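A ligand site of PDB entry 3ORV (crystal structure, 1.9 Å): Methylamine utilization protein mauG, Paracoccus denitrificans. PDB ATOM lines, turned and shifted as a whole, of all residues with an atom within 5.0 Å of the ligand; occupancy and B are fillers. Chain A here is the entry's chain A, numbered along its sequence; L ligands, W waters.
NH2 of Arg 96 is in salt-bridge range of O3 of the ligand. N of Trp 93 lies within hydrogen-bond range of O4 of the ligand (2.9 Å). A carbon (C25) of the ligand is covalently linked to the side-chain sulfur (SG) of Cys 34. The backbone NH of Phe 92 sits at hydrogen-bond distance from an oxygen (O2) of the ligand, at 2.7 Å. A carbon (C18) of the ligand is bonded to the side-chain sulfur (SG) of Cys 31, at 1.8 Å. An oxygen (O3) of the ligand is in salt-bridge range of the guanidinium group (NH1) of Arg 65, 2.8 Å away. The side-chain amino group of Lys 265 is in salt-bridge range of an oxygen (O1) of the ligand, 2.9 Å away. An iron atom (FE1) of the ligand is bound by a ring nitrogen (NE2) of His 35, at 2.2 Å.
NH2 of Arg 45 is in hydrogen-bond range of O of Val 55. N of Cys 31 lies close to O of Phe 18 (3.4 Å). The side-chain sulfur (SG) of Cys 34 is in hydrogen-bond range of the guanidinium group (NH2) of Arg 45, at 3.3 Å. The guanidinium group (NH2) of Arg 96 is in salt-bridge range of the side-chain carboxylate (OD2) of Asp 94 (2.9 Å). O of Trp 93 sits at hydrogen-bond distance from N of Lys 265. NE1 of Trp 93 is in hydrogen-bond range of O of Asn 66 (2.8 Å). The side-chain carboxylate of Asp 94 is in salt-bridge range of the guanidinium group of Arg 65 (2.9 Å). The backbone carbonyl oxygen of Pro 107 is in hydrogen-bond range of the backbone NH of Met 114.
N1 of the ligand sits close to NE2 of Gln 103 (3.1 Å). NE2 of Gln 29 touches C24 of the ligand, at 3.5 Å. O of Ser 30 touches C24 of the ligand, 3.6 Å away. CB of Ser 54 touches C25 of the ligand, at 3.7 Å. Val 55 touches the ligand. Gly 56 touches the ligand (CA to C26, 3.99 Å). Asn 66 touches the ligand (O to C32, 3.95 Å). Thr 67 touches the ligand. CD of Pro 68 touches C29 of the ligand (3.3 Å). Leu 70 touches the ligand. Gln 91 touches the ligand (NE2 to C11, 3.5 Å). Leu 100 touches the ligand. O of Ala 104 touches C19 of the ligand (3.6 Å). Pro 107 touches the ligand. Met 108 touches the ligand (CG to C19, 3.96 Å). Glu 113 touches the ligand. Met 114 touches the ligand. Gln 163 touches the ligand. The nearest printed residue that does not touch the ligand is Leu 159 (4.1 Å).
Water W6 lies within hydrogen-bond range of O1 of the ligand (2.6 Å) and NE2 of Gln 91 (3.0 Å). Water W7 lies within hydrogen-bond range of O of Thr 69 and O1 of the ligand. Water W5 bridges O2 of the ligand (2.9 Å) and NZ of Lys 265 (3.4 Å). Water W1 bridges N of Ser 54 and O of Arg 65. Water W4 lies within hydrogen-bond range of O of Val 112 (2.7 Å) and O of Ser 54 (2.9 Å).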
ATOM      1  N   PHE A  18     -19.777 -18.216 -18.457  1.00  0.00           N
ATOM      2  CA  PHE A  18     -19.504 -16.922 -19.041  1.00  0.00           C
ATOM      3  C   PHE A  18     -18.596 -17.026 -20.292  1.00  0.00           C
ATOM      4  O   PHE A  18     -18.716 -16.200 -21.190  1.00  0.00           O
ATOM      5  CB  PHE A  18     -18.754 -16.057 -18.006  1.00  0.00           C
ATOM      6  CG  PHE A  18     -18.569 -14.626 -18.426  1.00  0.00           C
ATOM      7  CD1 PHE A  18     -19.626 -13.725 -18.289  1.00  0.00           C
ATOM      8  CD2 PHE A  18     -17.335 -14.186 -18.949  1.00  0.00           C
ATOM      9  CE1 PHE A  18     -19.496 -12.397 -18.656  1.00  0.00           C
ATOM     10  CE2 PHE A  18     -17.207 -12.825 -19.341  1.00  0.00           C
ATOM     11  CZ  PHE A  18     -18.270 -11.955 -19.209  1.00  0.00           C
ATOM     12  N   GLN A  29     -20.213 -18.063 -30.087  1.00  0.00           N
ATOM     13  CA  GLN A  29     -20.008 -16.910 -29.217  1.00  0.00           C
ATOM     14  C   GLN A  29     -20.428 -17.161 -27.809  1.00  0.00           C
ATOM     15  O   GLN A  29     -21.358 -17.918 -27.572  1.00  0.00           O
ATOM     16  CB  GLN A  29     -20.525 -15.594 -29.830  1.00  0.00           C
ATOM     17  CG  GLN A  29     -21.862 -15.179 -29.512  1.00  0.00           C
ATOM     18  CD  GLN A  29     -22.228 -13.809 -30.151  1.00  0.00           C
ATOM     19  OE1 GLN A  29     -21.414 -13.072 -30.810  1.00  0.00           O
ATOM     20  NE2 GLN A  29     -23.452 -13.512 -30.024  1.00  0.00           N
ATOM     21  N   SER A  30     -19.689 -16.579 -26.879  1.00  0.00           N
ATOM     22  CA  SER A  30     -20.024 -16.674 -25.451  1.00  0.00           C
ATOM     23  C   SER A  30     -20.279 -15.222 -24.952  1.00  0.00           C
ATOM     24  O   SER A  30     -20.026 -14.225 -25.739  1.00  0.00           O
ATOM     25  CB  SER A  30     -18.876 -17.311 -24.660  1.00  0.00           C
ATOM     26  OG  SER A  30     -17.677 -16.470 -24.705  1.00  0.00           O
ATOM     27  N   CYS A  31     -20.691 -15.071 -23.692  1.00  0.00           N
ATOM     28  CA  CYS A  31     -20.766 -13.696 -23.087  1.00  0.00           C
ATOM     29  C   CYS A  31     -19.415 -12.986 -23.288  1.00  0.00           C
ATOM     30  O   CYS A  31     -19.365 -11.753 -23.540  1.00  0.00           O
ATOM     31  CB  CYS A  31     -20.992 -13.751 -21.565  1.00  0.00           C
ATOM     32  SG  CYS A  31     -22.369 -14.830 -20.959  1.00  0.00           S
ATOM     33  N   CYS A  34     -18.470 -10.795 -26.632  1.00  0.00           N
ATOM     34  CA  CYS A  34     -18.821  -9.376 -26.683  1.00  0.00           C
ATOM     35  C   CYS A  34     -18.351  -8.639 -25.420  1.00  0.00           C
ATOM     36  O   CYS A  34     -18.073  -7.427 -25.482  1.00  0.00           O
ATOM     37  CB  CYS A  34     -20.308  -9.197 -26.798  1.00  0.00           C
ATOM     38  SG  CYS A  34     -20.957  -9.881 -28.331  1.00  0.00           S
ATOM     39  N   HIS A  35     -18.279  -9.334 -24.300  1.00  0.00           N
ATOM     40  CA  HIS A  35     -17.765  -8.709 -23.045  1.00  0.00           C
ATOM     41  C   HIS A  35     -16.381  -9.234 -22.749  1.00  0.00           C
ATOM     42  O   HIS A  35     -16.173 -10.078 -21.857  1.00  0.00           O
ATOM     43  CB  HIS A  35     -18.712  -9.001 -21.884  1.00  0.00           C
ATOM     44  CG  HIS A  35     -20.068  -8.415 -22.084  1.00  0.00           C
ATOM     45  ND1 HIS A  35     -20.320  -7.064 -21.921  1.00  0.00           N
ATOM     46  CD2 HIS A  35     -21.262  -8.989 -22.414  1.00  0.00           C
ATOM     47  CE1 HIS A  35     -21.608  -6.833 -22.139  1.00  0.00           C
ATOM     48  NE2 HIS A  35     -22.210  -7.984 -22.398  1.00  0.00           N
ATOM     49  N   ARG A  45     -14.155  -6.135 -31.414  1.00  0.00           N
ATOM     50  CA  ARG A  45     -14.297  -6.493 -32.799  1.00  0.00           C
ATOM     51  C   ARG A  45     -14.873  -5.381 -33.704  1.00  0.00           C
ATOM     52  O   ARG A  45     -15.746  -4.608 -33.248  1.00  0.00           O
ATOM     53  CB  ARG A  45     -15.205  -7.736 -32.851  1.00  0.00           C
ATOM     54  CG  ARG A  45     -14.600  -8.942 -32.063  1.00  0.00           C
ATOM     55  CD  ARG A  45     -15.587 -10.101 -32.024  1.00  0.00           C
ATOM     56  NE  ARG A  45     -16.865  -9.665 -31.448  1.00  0.00           N
ATOM     57  CZ  ARG A  45     -18.054 -10.226 -31.688  1.00  0.00           C
ATOM     58  NH1 ARG A  45     -18.180 -11.223 -32.547  1.00  0.00           N
ATOM     59  NH2 ARG A  45     -19.155  -9.734 -31.096  1.00  0.00           N
ATOM     60  N   SER A  54     -22.304  -4.522 -31.803  1.00  0.00           N
ATOM     61  CA  SER A  54     -21.646  -5.859 -31.865  1.00  0.00           C
ATOM     62  C   SER A  54     -22.382  -6.808 -32.844  1.00  0.00           C
ATOM     63  O   SER A  54     -23.595  -6.725 -33.040  1.00  0.00           O
ATOM     64  CB  SER A  54     -21.650  -6.517 -30.477  1.00  0.00           C
ATOM     65  OG  SER A  54     -20.778  -5.835 -29.577  1.00  0.00           O
ATOM     66  N   VAL A  55     -21.644  -7.756 -33.370  1.00  0.00           N
ATOM     67  CA  VAL A  55     -22.236  -8.724 -34.307  1.00  0.00           C
ATOM     68  C   VAL A  55     -22.583  -9.974 -33.527  1.00  0.00           C
ATOM     69  O   VAL A  55     -21.810 -10.386 -32.648  1.00  0.00           O
ATOM     70  CB  VAL A  55     -21.219  -9.078 -35.362  1.00  0.00           C
ATOM     71  CG1 VAL A  55     -21.786 -10.162 -36.319  1.00  0.00           C
ATOM     72  CG2 VAL A  55     -20.860  -7.792 -36.163  1.00  0.00           C
ATOM     73  N   GLY A  56     -23.756 -10.537 -33.800  1.00  0.00           N
ATOM     74  CA  GLY A  56     -24.289 -11.710 -33.040  1.00  0.00           C
ATOM     75  C   GLY A  56     -23.714 -13.033 -33.570  1.00  0.00           C
ATOM     76  O   GLY A  56     -22.849 -13.056 -34.481  1.00  0.00           O
ATOM     77  N   ARG A  65     -27.366  -0.990 -30.202  1.00  0.00           N
ATOM     78  CA  ARG A  65     -26.766  -0.238 -29.056  1.00  0.00           C
ATOM     79  C   ARG A  65     -25.353  -0.710 -28.805  1.00  0.00           C
ATOM     80  O   ARG A  65     -25.040  -1.850 -29.149  1.00  0.00           O
ATOM     81  CB  ARG A  65     -27.593  -0.469 -27.773  1.00  0.00           C
ATOM     82  CG  ARG A  65     -28.925   0.321 -27.871  1.00  0.00           C
ATOM     83  CD  ARG A  65     -29.657   0.210 -26.608  1.00  0.00           C
ATOM     84  NE  ARG A  65     -30.924   0.894 -26.621  1.00  0.00           N
ATOM     85  CZ  ARG A  65     -31.965   0.455 -25.912  1.00  0.00           C
ATOM     86  NH1 ARG A  65     -31.834  -0.633 -25.168  1.00  0.00           N
ATOM     87  NH2 ARG A  65     -33.110   1.139 -25.906  1.00  0.00           N
ATOM     88  N   ASN A  66     -24.522   0.137 -28.209  1.00  0.00           N
ATOM     89  CA  ASN A  66     -23.111  -0.227 -27.905  1.00  0.00           C
ATOM     90  C   ASN A  66     -23.060  -1.203 -26.730  1.00  0.00           C
ATOM     91  O   ASN A  66     -23.787  -1.026 -25.737  1.00  0.00           O
ATOM     92  CB  ASN A  66     -22.371   1.090 -27.578  1.00  0.00           C
ATOM     93  CG  ASN A  66     -20.933   0.892 -27.301  1.00  0.00           C
ATOM     94  OD1 ASN A  66     -20.487   1.139 -26.192  1.00  0.00           O
ATOM     95  ND2 ASN A  66     -20.177   0.446 -28.330  1.00  0.00           N
ATOM     96  N   THR A  67     -22.213  -2.229 -26.800  1.00  0.00           N
ATOM     97  CA  THR A  67     -22.087  -3.207 -25.719  1.00  0.00           C
ATOM     98  C   THR A  67     -21.390  -2.550 -24.508  1.00  0.00           C
ATOM     99  O   THR A  67     -20.245  -2.055 -24.661  1.00  0.00           O
ATOM    100  CB  THR A  67     -21.227  -4.401 -26.162  1.00  0.00           C
ATOM    101  OG1 THR A  67     -21.916  -5.106 -27.174  1.00  0.00           O
ATOM    102  CG2 THR A  67     -20.901  -5.354 -25.007  1.00  0.00           C
ATOM    103  N   PRO A  68     -22.028  -2.523 -23.337  1.00  0.00           N
ATOM    104  CA  PRO A  68     -21.394  -1.814 -22.197  1.00  0.00           C
ATOM    105  C   PRO A  68     -20.459  -2.738 -21.385  1.00  0.00           C
ATOM    106  O   PRO A  68     -20.597  -3.997 -21.418  1.00  0.00           O
ATOM    107  CB  PRO A  68     -22.620  -1.335 -21.385  1.00  0.00           C
ATOM    108  CG  PRO A  68     -23.606  -2.566 -21.554  1.00  0.00           C
ATOM    109  CD  PRO A  68     -23.435  -2.926 -23.027  1.00  0.00           C
ATOM    110  N   THR A  69     -19.550  -2.156 -20.631  1.00  0.00           N
ATOM    111  CA  THR A  69     -18.867  -2.924 -19.555  1.00  0.00           C
ATOM    112  C   THR A  69     -19.725  -3.665 -18.563  1.00  0.00           C
ATOM    113  O   THR A  69     -20.813  -3.205 -18.142  1.00  0.00           O
ATOM    114  CB  THR A  69     -17.777  -2.035 -18.804  1.00  0.00           C
ATOM    115  OG1 THR A  69     -16.929  -2.875 -18.027  1.00  0.00           O
ATOM    116  CG2 THR A  69     -18.432  -0.981 -17.865  1.00  0.00           C
ATOM    117  N   LEU A  70     -19.254  -4.828 -18.155  1.00  0.00           N
ATOM    118  CA  LEU A  70     -19.853  -5.495 -17.009  1.00  0.00           C
ATOM    119  C   LEU A  70     -19.141  -5.155 -15.705  1.00  0.00           C
ATOM    120  O   LEU A  70     -19.578  -5.545 -14.607  1.00  0.00           O
ATOM    121  CB  LEU A  70     -19.822  -7.024 -17.224  1.00  0.00           C
ATOM    122  CG  LEU A  70     -20.462  -7.499 -18.540  1.00  0.00           C
ATOM    123  CD1 LEU A  70     -20.537  -9.026 -18.536  1.00  0.00           C
ATOM    124  CD2 LEU A  70     -21.861  -6.924 -18.641  1.00  0.00           C
ATOM    125  N   ALA A  73     -21.134  -3.501 -12.644  1.00  0.00           N
ATOM    126  CA  ALA A  73     -22.578  -3.554 -12.924  1.00  0.00           C
ATOM    127  C   ALA A  73     -23.310  -4.150 -11.700  1.00  0.00           C
ATOM    128  O   ALA A  73     -24.509  -3.877 -11.469  1.00  0.00           O
ATOM    129  CB  ALA A  73     -22.861  -4.334 -14.206  1.00  0.00           C
ATOM    130  N   GLN A  91     -30.838  -2.912 -15.444  1.00  0.00           N
ATOM    131  CA  GLN A  91     -29.746  -3.292 -16.356  1.00  0.00           C
ATOM    132  C   GLN A  91     -30.214  -3.075 -17.801  1.00  0.00           C
ATOM    133  O   GLN A  91     -31.457  -3.127 -18.075  1.00  0.00           O
ATOM    134  CB  GLN A  91     -29.324  -4.765 -16.086  1.00  0.00           C
ATOM    135  CG  GLN A  91     -28.798  -5.072 -14.636  1.00  0.00           C
ATOM    136  CD  GLN A  91     -27.409  -4.466 -14.312  1.00  0.00           C
ATOM    137  OE1 GLN A  91     -27.071  -4.264 -13.144  1.00  0.00           O
ATOM    138  NE2 GLN A  91     -26.639  -4.141 -15.328  1.00  0.00           N
ATOM    139  N   PHE A  92     -29.245  -2.916 -18.706  1.00  0.00           N
ATOM    140  CA  PHE A  92     -29.418  -2.489 -20.123  1.00  0.00           C
ATOM    141  C   PHE A  92     -29.420  -0.931 -20.117  1.00  0.00           C
ATOM    142  O   PHE A  92     -29.708  -0.301 -19.072  1.00  0.00           O
ATOM    143  CB  PHE A  92     -30.662  -3.051 -20.812  1.00  0.00           C
ATOM    144  CG  PHE A  92     -30.573  -4.543 -21.148  1.00  0.00           C
ATOM    145  CD1 PHE A  92     -29.532  -5.043 -21.914  1.00  0.00           C
ATOM    146  CD2 PHE A  92     -31.542  -5.442 -20.736  1.00  0.00           C
ATOM    147  CE1 PHE A  92     -29.486  -6.431 -22.264  1.00  0.00           C
ATOM    148  CE2 PHE A  92     -31.463  -6.787 -21.109  1.00  0.00           C
ATOM    149  CZ  PHE A  92     -30.438  -7.242 -21.857  1.00  0.00           C
ATOM    150  N   TRP A  93     -29.137  -0.337 -21.274  1.00  0.00           N
ATOM    151  CA  TRP A  93     -29.099   1.107 -21.380  1.00  0.00           C
ATOM    152  C   TRP A  93     -30.495   1.668 -21.116  1.00  0.00           C
ATOM    153  O   TRP A  93     -30.594   2.812 -20.764  1.00  0.00           O
ATOM    154  CB  TRP A  93     -28.672   1.496 -22.801  1.00  0.00           C
ATOM    155  CG  TRP A  93     -27.168   1.334 -23.134  1.00  0.00           C
ATOM    156  CD1 TRP A  93     -26.563   0.314 -23.808  1.00  0.00           C
ATOM    157  CD2 TRP A  93     -26.123   2.289 -22.842  1.00  0.00           C
ATOM    158  NE1 TRP A  93     -25.188   0.535 -23.933  1.00  0.00           N
ATOM    159  CE2 TRP A  93     -24.904   1.759 -23.364  1.00  0.00           C
ATOM    160  CE3 TRP A  93     -26.112   3.551 -22.236  1.00  0.00           C
ATOM    161  CZ2 TRP A  93     -23.692   2.433 -23.263  1.00  0.00           C
ATOM    162  CZ3 TRP A  93     -24.871   4.242 -22.119  1.00  0.00           C
ATOM    163  CH2 TRP A  93     -23.688   3.705 -22.664  1.00  0.00           C
ATOM    164  N   ASP A  94     -31.564   0.905 -21.405  1.00  0.00           N
ATOM    165  CA  ASP A  94     -32.955   1.383 -21.139  1.00  0.00           C
ATOM    166  C   ASP A  94     -33.571   0.783 -19.870  1.00  0.00           C
ATOM    167  O   ASP A  94     -34.760   0.935 -19.649  1.00  0.00           O
ATOM    168  CB  ASP A  94     -33.917   1.079 -22.314  1.00  0.00           C
ATOM    169  CG  ASP A  94     -33.915  -0.368 -22.705  1.00  0.00           C
ATOM    170  OD1 ASP A  94     -34.420  -0.683 -23.809  1.00  0.00           O
ATOM    171  OD2 ASP A  94     -33.320  -1.209 -21.958  1.00  0.00           O
ATOM    172  N   ARG A  96     -34.557  -2.107 -19.024  1.00  0.00           N
ATOM    173  CA  ARG A  96     -35.649  -3.047 -19.169  1.00  0.00           C
ATOM    174  C   ARG A  96     -35.499  -4.350 -18.411  1.00  0.00           C
ATOM    175  O   ARG A  96     -36.490  -5.101 -18.302  1.00  0.00           O
ATOM    176  CB  ARG A  96     -35.954  -3.262 -20.639  1.00  0.00           C
ATOM    177  CG  ARG A  96     -34.903  -4.109 -21.354  1.00  0.00           C
ATOM    178  CD  ARG A  96     -35.191  -4.284 -22.873  1.00  0.00           C
ATOM    179  NE  ARG A  96     -34.209  -5.140 -23.568  1.00  0.00           N
ATOM    180  CZ  ARG A  96     -33.052  -4.718 -24.006  1.00  0.00           C
ATOM    181  NH1 ARG A  96     -32.252  -5.551 -24.684  1.00  0.00           N
ATOM    182  NH2 ARG A  96     -32.696  -3.452 -23.767  1.00  0.00           N
ATOM    183  N   LEU A 100     -29.338  -8.217 -12.435  1.00  0.00           N
ATOM    184  CA  LEU A 100     -28.413  -9.032 -13.274  1.00  0.00           C
ATOM    185  C   LEU A 100     -28.972 -10.379 -13.547  1.00  0.00           C
ATOM    186  O   LEU A 100     -28.696 -10.958 -14.623  1.00  0.00           O
ATOM    187  CB  LEU A 100     -27.060  -9.230 -12.592  1.00  0.00           C
ATOM    188  CG  LEU A 100     -26.142  -7.998 -12.510  1.00  0.00           C
ATOM    189  CD1 LEU A 100     -24.963  -8.378 -11.615  1.00  0.00           C
ATOM    190  CD2 LEU A 100     -25.721  -7.661 -13.949  1.00  0.00           C
ATOM    191  N   GLN A 103     -31.421 -10.088 -16.313  1.00  0.00           N
ATOM    192  CA  GLN A 103     -30.803  -9.716 -17.581  1.00  0.00           C
ATOM    193  C   GLN A 103     -30.172 -10.960 -18.233  1.00  0.00           C
ATOM    194  O   GLN A 103     -30.152 -11.042 -19.454  1.00  0.00           O
ATOM    195  CB  GLN A 103     -29.706  -8.712 -17.337  1.00  0.00           C
ATOM    196  CG  GLN A 103     -29.048  -8.160 -18.641  1.00  0.00           C
ATOM    197  CD  GLN A 103     -28.002  -9.113 -19.227  1.00  0.00           C
ATOM    198  OE1 GLN A 103     -27.437 -10.011 -18.518  1.00  0.00           O
ATOM    199  NE2 GLN A 103     -27.691  -8.915 -20.505  1.00  0.00           N
ATOM    200  N   ALA A 104     -29.644 -11.898 -17.427  1.00  0.00           N
ATOM    201  CA  ALA A 104     -28.642 -12.887 -17.985  1.00  0.00           C
ATOM    202  C   ALA A 104     -29.201 -13.788 -19.087  1.00  0.00           C
ATOM    203  O   ALA A 104     -28.464 -14.154 -20.028  1.00  0.00           O
ATOM    204  CB  ALA A 104     -27.992 -13.728 -16.883  1.00  0.00           C
ATOM    205  N   PRO A 107     -29.556 -12.226 -23.530  1.00  0.00           N
ATOM    206  CA  PRO A 107     -28.721 -12.350 -24.770  1.00  0.00           C
ATOM    207  C   PRO A 107     -28.749 -13.797 -25.342  1.00  0.00           C
ATOM    208  O   PRO A 107     -28.573 -14.004 -26.557  1.00  0.00           O
ATOM    209  CB  PRO A 107     -27.283 -12.006 -24.294  1.00  0.00           C
ATOM    210  CG  PRO A 107     -27.368 -11.472 -22.885  1.00  0.00           C
ATOM    211  CD  PRO A 107     -28.808 -11.611 -22.395  1.00  0.00           C
ATOM    212  N   MET A 108     -28.954 -14.781 -24.456  1.00  0.00           N
ATOM    213  CA  MET A 108     -28.960 -16.187 -24.856  1.00  0.00           C
ATOM    214  C   MET A 108     -30.051 -16.455 -25.906  1.00  0.00           C
ATOM    215  O   MET A 108     -29.796 -17.174 -26.877  1.00  0.00           O
ATOM    216  CB  MET A 108     -29.175 -17.092 -23.638  1.00  0.00           C
ATOM    217  CG  MET A 108     -27.953 -17.225 -22.703  1.00  0.00           C
ATOM    218  SD  MET A 108     -28.417 -18.358 -21.316  1.00  0.00           S
ATOM    219  CE  MET A 108     -27.524 -17.670 -19.899  1.00  0.00           C
ATOM    220  N   VAL A 112     -30.456 -11.533 -32.515  1.00  0.00           N
ATOM    221  CA  VAL A 112     -29.343 -10.759 -33.055  1.00  0.00           C
ATOM    222  C   VAL A 112     -28.153 -10.899 -32.134  1.00  0.00           C
ATOM    223  O   VAL A 112     -27.083 -10.319 -32.399  1.00  0.00           O
ATOM    224  CB  VAL A 112     -29.653  -9.271 -33.372  1.00  0.00           C
ATOM    225  CG1 VAL A 112     -31.085  -9.129 -34.014  1.00  0.00           C
ATOM    226  CG2 VAL A 112     -29.504  -8.444 -32.198  1.00  0.00           C
ATOM    227  N   GLU A 113     -28.304 -11.671 -31.036  1.00  0.00           N
ATOM    228  CA  GLU A 113     -27.093 -11.952 -30.213  1.00  0.00           C
ATOM    229  C   GLU A 113     -26.764 -13.452 -30.237  1.00  0.00           C
ATOM    230  O   GLU A 113     -26.418 -13.973 -31.290  1.00  0.00           O
ATOM    231  CB  GLU A 113     -27.238 -11.362 -28.794  1.00  0.00           C
ATOM    232  CG  GLU A 113     -27.415  -9.797 -28.904  1.00  0.00           C
ATOM    233  CD  GLU A 113     -27.588  -9.086 -27.523  1.00  0.00           C
ATOM    234  OE1 GLU A 113     -27.874  -9.791 -26.522  1.00  0.00           O
ATOM    235  OE2 GLU A 113     -27.427  -7.815 -27.447  1.00  0.00           O
ATOM    236  N   MET A 114     -26.960 -14.175 -29.126  1.00  0.00           N
ATOM    237  CA  MET A 114     -26.553 -15.568 -29.088  1.00  0.00           C
ATOM    238  C   MET A 114     -27.563 -16.469 -29.817  1.00  0.00           C
ATOM    239  O   MET A 114     -27.199 -17.547 -30.243  1.00  0.00           O
ATOM    240  CB  MET A 114     -26.304 -15.987 -27.647  1.00  0.00           C
ATOM    241  CG  MET A 114     -25.222 -15.094 -26.962  1.00  0.00           C
ATOM    242  SD  MET A 114     -24.951 -15.365 -25.180  1.00  0.00           S
ATOM    243  CE  MET A 114     -23.753 -16.676 -25.213  1.00  0.00           C
ATOM    244  N   LEU A 159     -24.461 -16.903 -13.481  1.00  0.00           N
ATOM    245  CA  LEU A 159     -23.835 -15.791 -14.224  1.00  0.00           C
ATOM    246  C   LEU A 159     -23.935 -14.487 -13.387  1.00  0.00           C
ATOM    247  O   LEU A 159     -22.997 -13.706 -13.312  1.00  0.00           O
ATOM    248  CB  LEU A 159     -24.489 -15.624 -15.562  1.00  0.00           C
ATOM    249  CG  LEU A 159     -23.993 -16.657 -16.604  1.00  0.00           C
ATOM    250  CD1 LEU A 159     -25.020 -16.620 -17.725  1.00  0.00           C
ATOM    251  CD2 LEU A 159     -22.625 -16.344 -17.155  1.00  0.00           C
ATOM    252  N   GLN A 163     -20.732 -12.349 -11.835  1.00  0.00           N
ATOM    253  CA  GLN A 163     -20.559 -10.910 -12.059  1.00  0.00           C
ATOM    254  C   GLN A 163     -20.516 -10.090 -10.784  1.00  0.00           C
ATOM    255  O   GLN A 163     -20.055  -8.933 -10.839  1.00  0.00           O
ATOM    256  CB  GLN A 163     -21.653 -10.336 -13.009  1.00  0.00           C
ATOM    257  CG  GLN A 163     -21.613 -10.857 -14.462  1.00  0.00           C
ATOM    258  CD  GLN A 163     -22.881 -10.431 -15.223  1.00  0.00           C
ATOM    259  OE1 GLN A 163     -23.878 -11.174 -15.216  1.00  0.00           O
ATOM    260  NE2 GLN A 163     -22.882  -9.241 -15.807  1.00  0.00           N
ATOM    261  N   LYS A 265     -29.841   5.032 -19.242  1.00  0.00           N
ATOM    262  CA  LYS A 265     -29.186   4.908 -17.919  1.00  0.00           C
ATOM    263  C   LYS A 265     -27.821   5.582 -17.926  1.00  0.00           C
ATOM    264  O   LYS A 265     -27.055   5.427 -18.827  1.00  0.00           O
ATOM    265  CB  LYS A 265     -29.054   3.445 -17.482  1.00  0.00           C
ATOM    266  CG  LYS A 265     -28.377   3.219 -16.119  1.00  0.00           C
ATOM    267  CD  LYS A 265     -28.511   1.703 -15.643  1.00  0.00           C
ATOM    268  CE  LYS A 265     -27.919   0.670 -16.650  1.00  0.00           C
ATOM    269  NZ  LYS A 265     -26.456   0.683 -16.957  1.00  0.00           N
HETATM  270 FE1  LIG L   1     -24.265  -8.443 -22.838  1.00  0.00          FE
HETATM  271  C1  LIG L   1     -25.706  -5.487 -22.018  1.00  0.00           C
HETATM  272  C2  LIG L   1     -24.386  -9.504 -19.477  1.00  0.00           C
HETATM  273  C3  LIG L   1     -23.908 -11.682 -23.803  1.00  0.00           C
HETATM  274  C4  LIG L   1     -23.863  -7.354 -26.151  1.00  0.00           C
HETATM  275  N1  LIG L   1     -24.880  -7.662 -21.034  1.00  0.00           N
HETATM  276  C5  LIG L   1     -25.436  -6.431 -20.887  1.00  0.00           C
HETATM  277  C6  LIG L   1     -25.660  -6.069 -19.476  1.00  0.00           C
HETATM  278  C7  LIG L   1     -25.307  -7.202 -18.737  1.00  0.00           C
HETATM  279  C8  LIG L   1     -24.841  -8.160 -19.788  1.00  0.00           C
HETATM  280  C9  LIG L   1     -25.276  -7.437 -17.232  1.00  0.00           C
HETATM  281  C10 LIG L   1     -26.194  -4.733 -18.972  1.00  0.00           C
HETATM  282  C11 LIG L   1     -25.056  -3.847 -18.474  1.00  0.00           C
HETATM  283  C12 LIG L   1     -25.545  -2.389 -18.242  1.00  0.00           C
HETATM  284  O1  LIG L   1     -24.776  -1.609 -17.662  1.00  0.00           O
HETATM  285  O2  LIG L   1     -26.696  -2.008 -18.554  1.00  0.00           O
HETATM  286  N2  LIG L   1     -24.243 -10.283 -21.824  1.00  0.00           N
HETATM  287  C13 LIG L   1     -24.269 -10.544 -20.518  1.00  0.00           C
HETATM  288  C14 LIG L   1     -24.085 -12.005 -20.172  1.00  0.00           C
HETATM  289  C15 LIG L   1     -23.953 -12.638 -21.404  1.00  0.00           C
HETATM  290  C16 LIG L   1     -23.995 -11.504 -22.370  1.00  0.00           C
HETATM  291  C17 LIG L   1     -24.092 -12.553 -18.753  1.00  0.00           C
HETATM  292  C18 LIG L   1     -23.811 -14.148 -21.724  1.00  0.00           C
HETATM  293  C19 LIG L   1     -25.157 -14.769 -21.355  1.00  0.00           C
HETATM  294  N3  LIG L   1     -23.972  -9.356 -24.693  1.00  0.00           N
HETATM  295  C20 LIG L   1     -23.737 -10.667 -24.882  1.00  0.00           C
HETATM  296  C21 LIG L   1     -23.270 -10.989 -26.259  1.00  0.00           C
HETATM  297  C22 LIG L   1     -23.261  -9.757 -26.922  1.00  0.00           C
HETATM  298  C23 LIG L   1     -23.670  -8.805 -25.882  1.00  0.00           C
HETATM  299  C24 LIG L   1     -22.853 -12.352 -26.806  1.00  0.00           C
HETATM  300  C25 LIG L   1     -22.828  -9.376 -28.358  1.00  0.00           C
HETATM  301  C26 LIG L   1     -23.606 -10.032 -29.483  1.00  0.00           C
HETATM  302  N4  LIG L   1     -24.674  -6.691 -23.888  1.00  0.00           N
HETATM  303  C27 LIG L   1     -24.603  -6.468 -25.219  1.00  0.00           C
HETATM  304  C28 LIG L   1     -25.257  -5.225 -25.660  1.00  0.00           C
HETATM  305  C29 LIG L   1     -25.812  -4.687 -24.503  1.00  0.00           C
HETATM  306  C30 LIG L   1     -25.410  -5.641 -23.441  1.00  0.00           C
HETATM  307  C31 LIG L   1     -25.352  -4.695 -27.074  1.00  0.00           C
HETATM  308  C32 LIG L   1     -26.637  -3.428 -24.415  1.00  0.00           C
HETATM  309  C33 LIG L   1     -28.011  -3.801 -24.941  1.00  0.00           C
HETATM  310  C34 LIG L   1     -29.102  -2.794 -24.589  1.00  0.00           C
HETATM  311  O3  LIG L   1     -30.218  -2.945 -25.101  1.00  0.00           O
HETATM  312  O4  LIG L   1     -28.937  -1.890 -23.736  1.00  0.00           O
HETATM  313  O   HOH W   1     -24.681  -4.418 -30.383  1.00  0.00           O
HETATM  314  O   HOH W   2     -30.398  -3.527 -27.580  1.00  0.00           O
HETATM  315  O   HOH W   3     -26.522  -6.591 -29.619  1.00  0.00           O
HETATM  316  O   HOH W   4     -25.646  -8.195 -31.649  1.00  0.00           O
HETATM  317  O   HOH W   5     -25.774   0.127 -20.232  1.00  0.00           O
HETATM  318  O   HOH W   6     -24.787  -1.747 -15.041  1.00  0.00           O
HETATM  319  O   HOH W   7     -22.190  -1.044 -17.511  1.00  0.00           O
HETATM  320  O   HOH W   8     -27.641  -7.896 -24.574  1.00  0.00           O
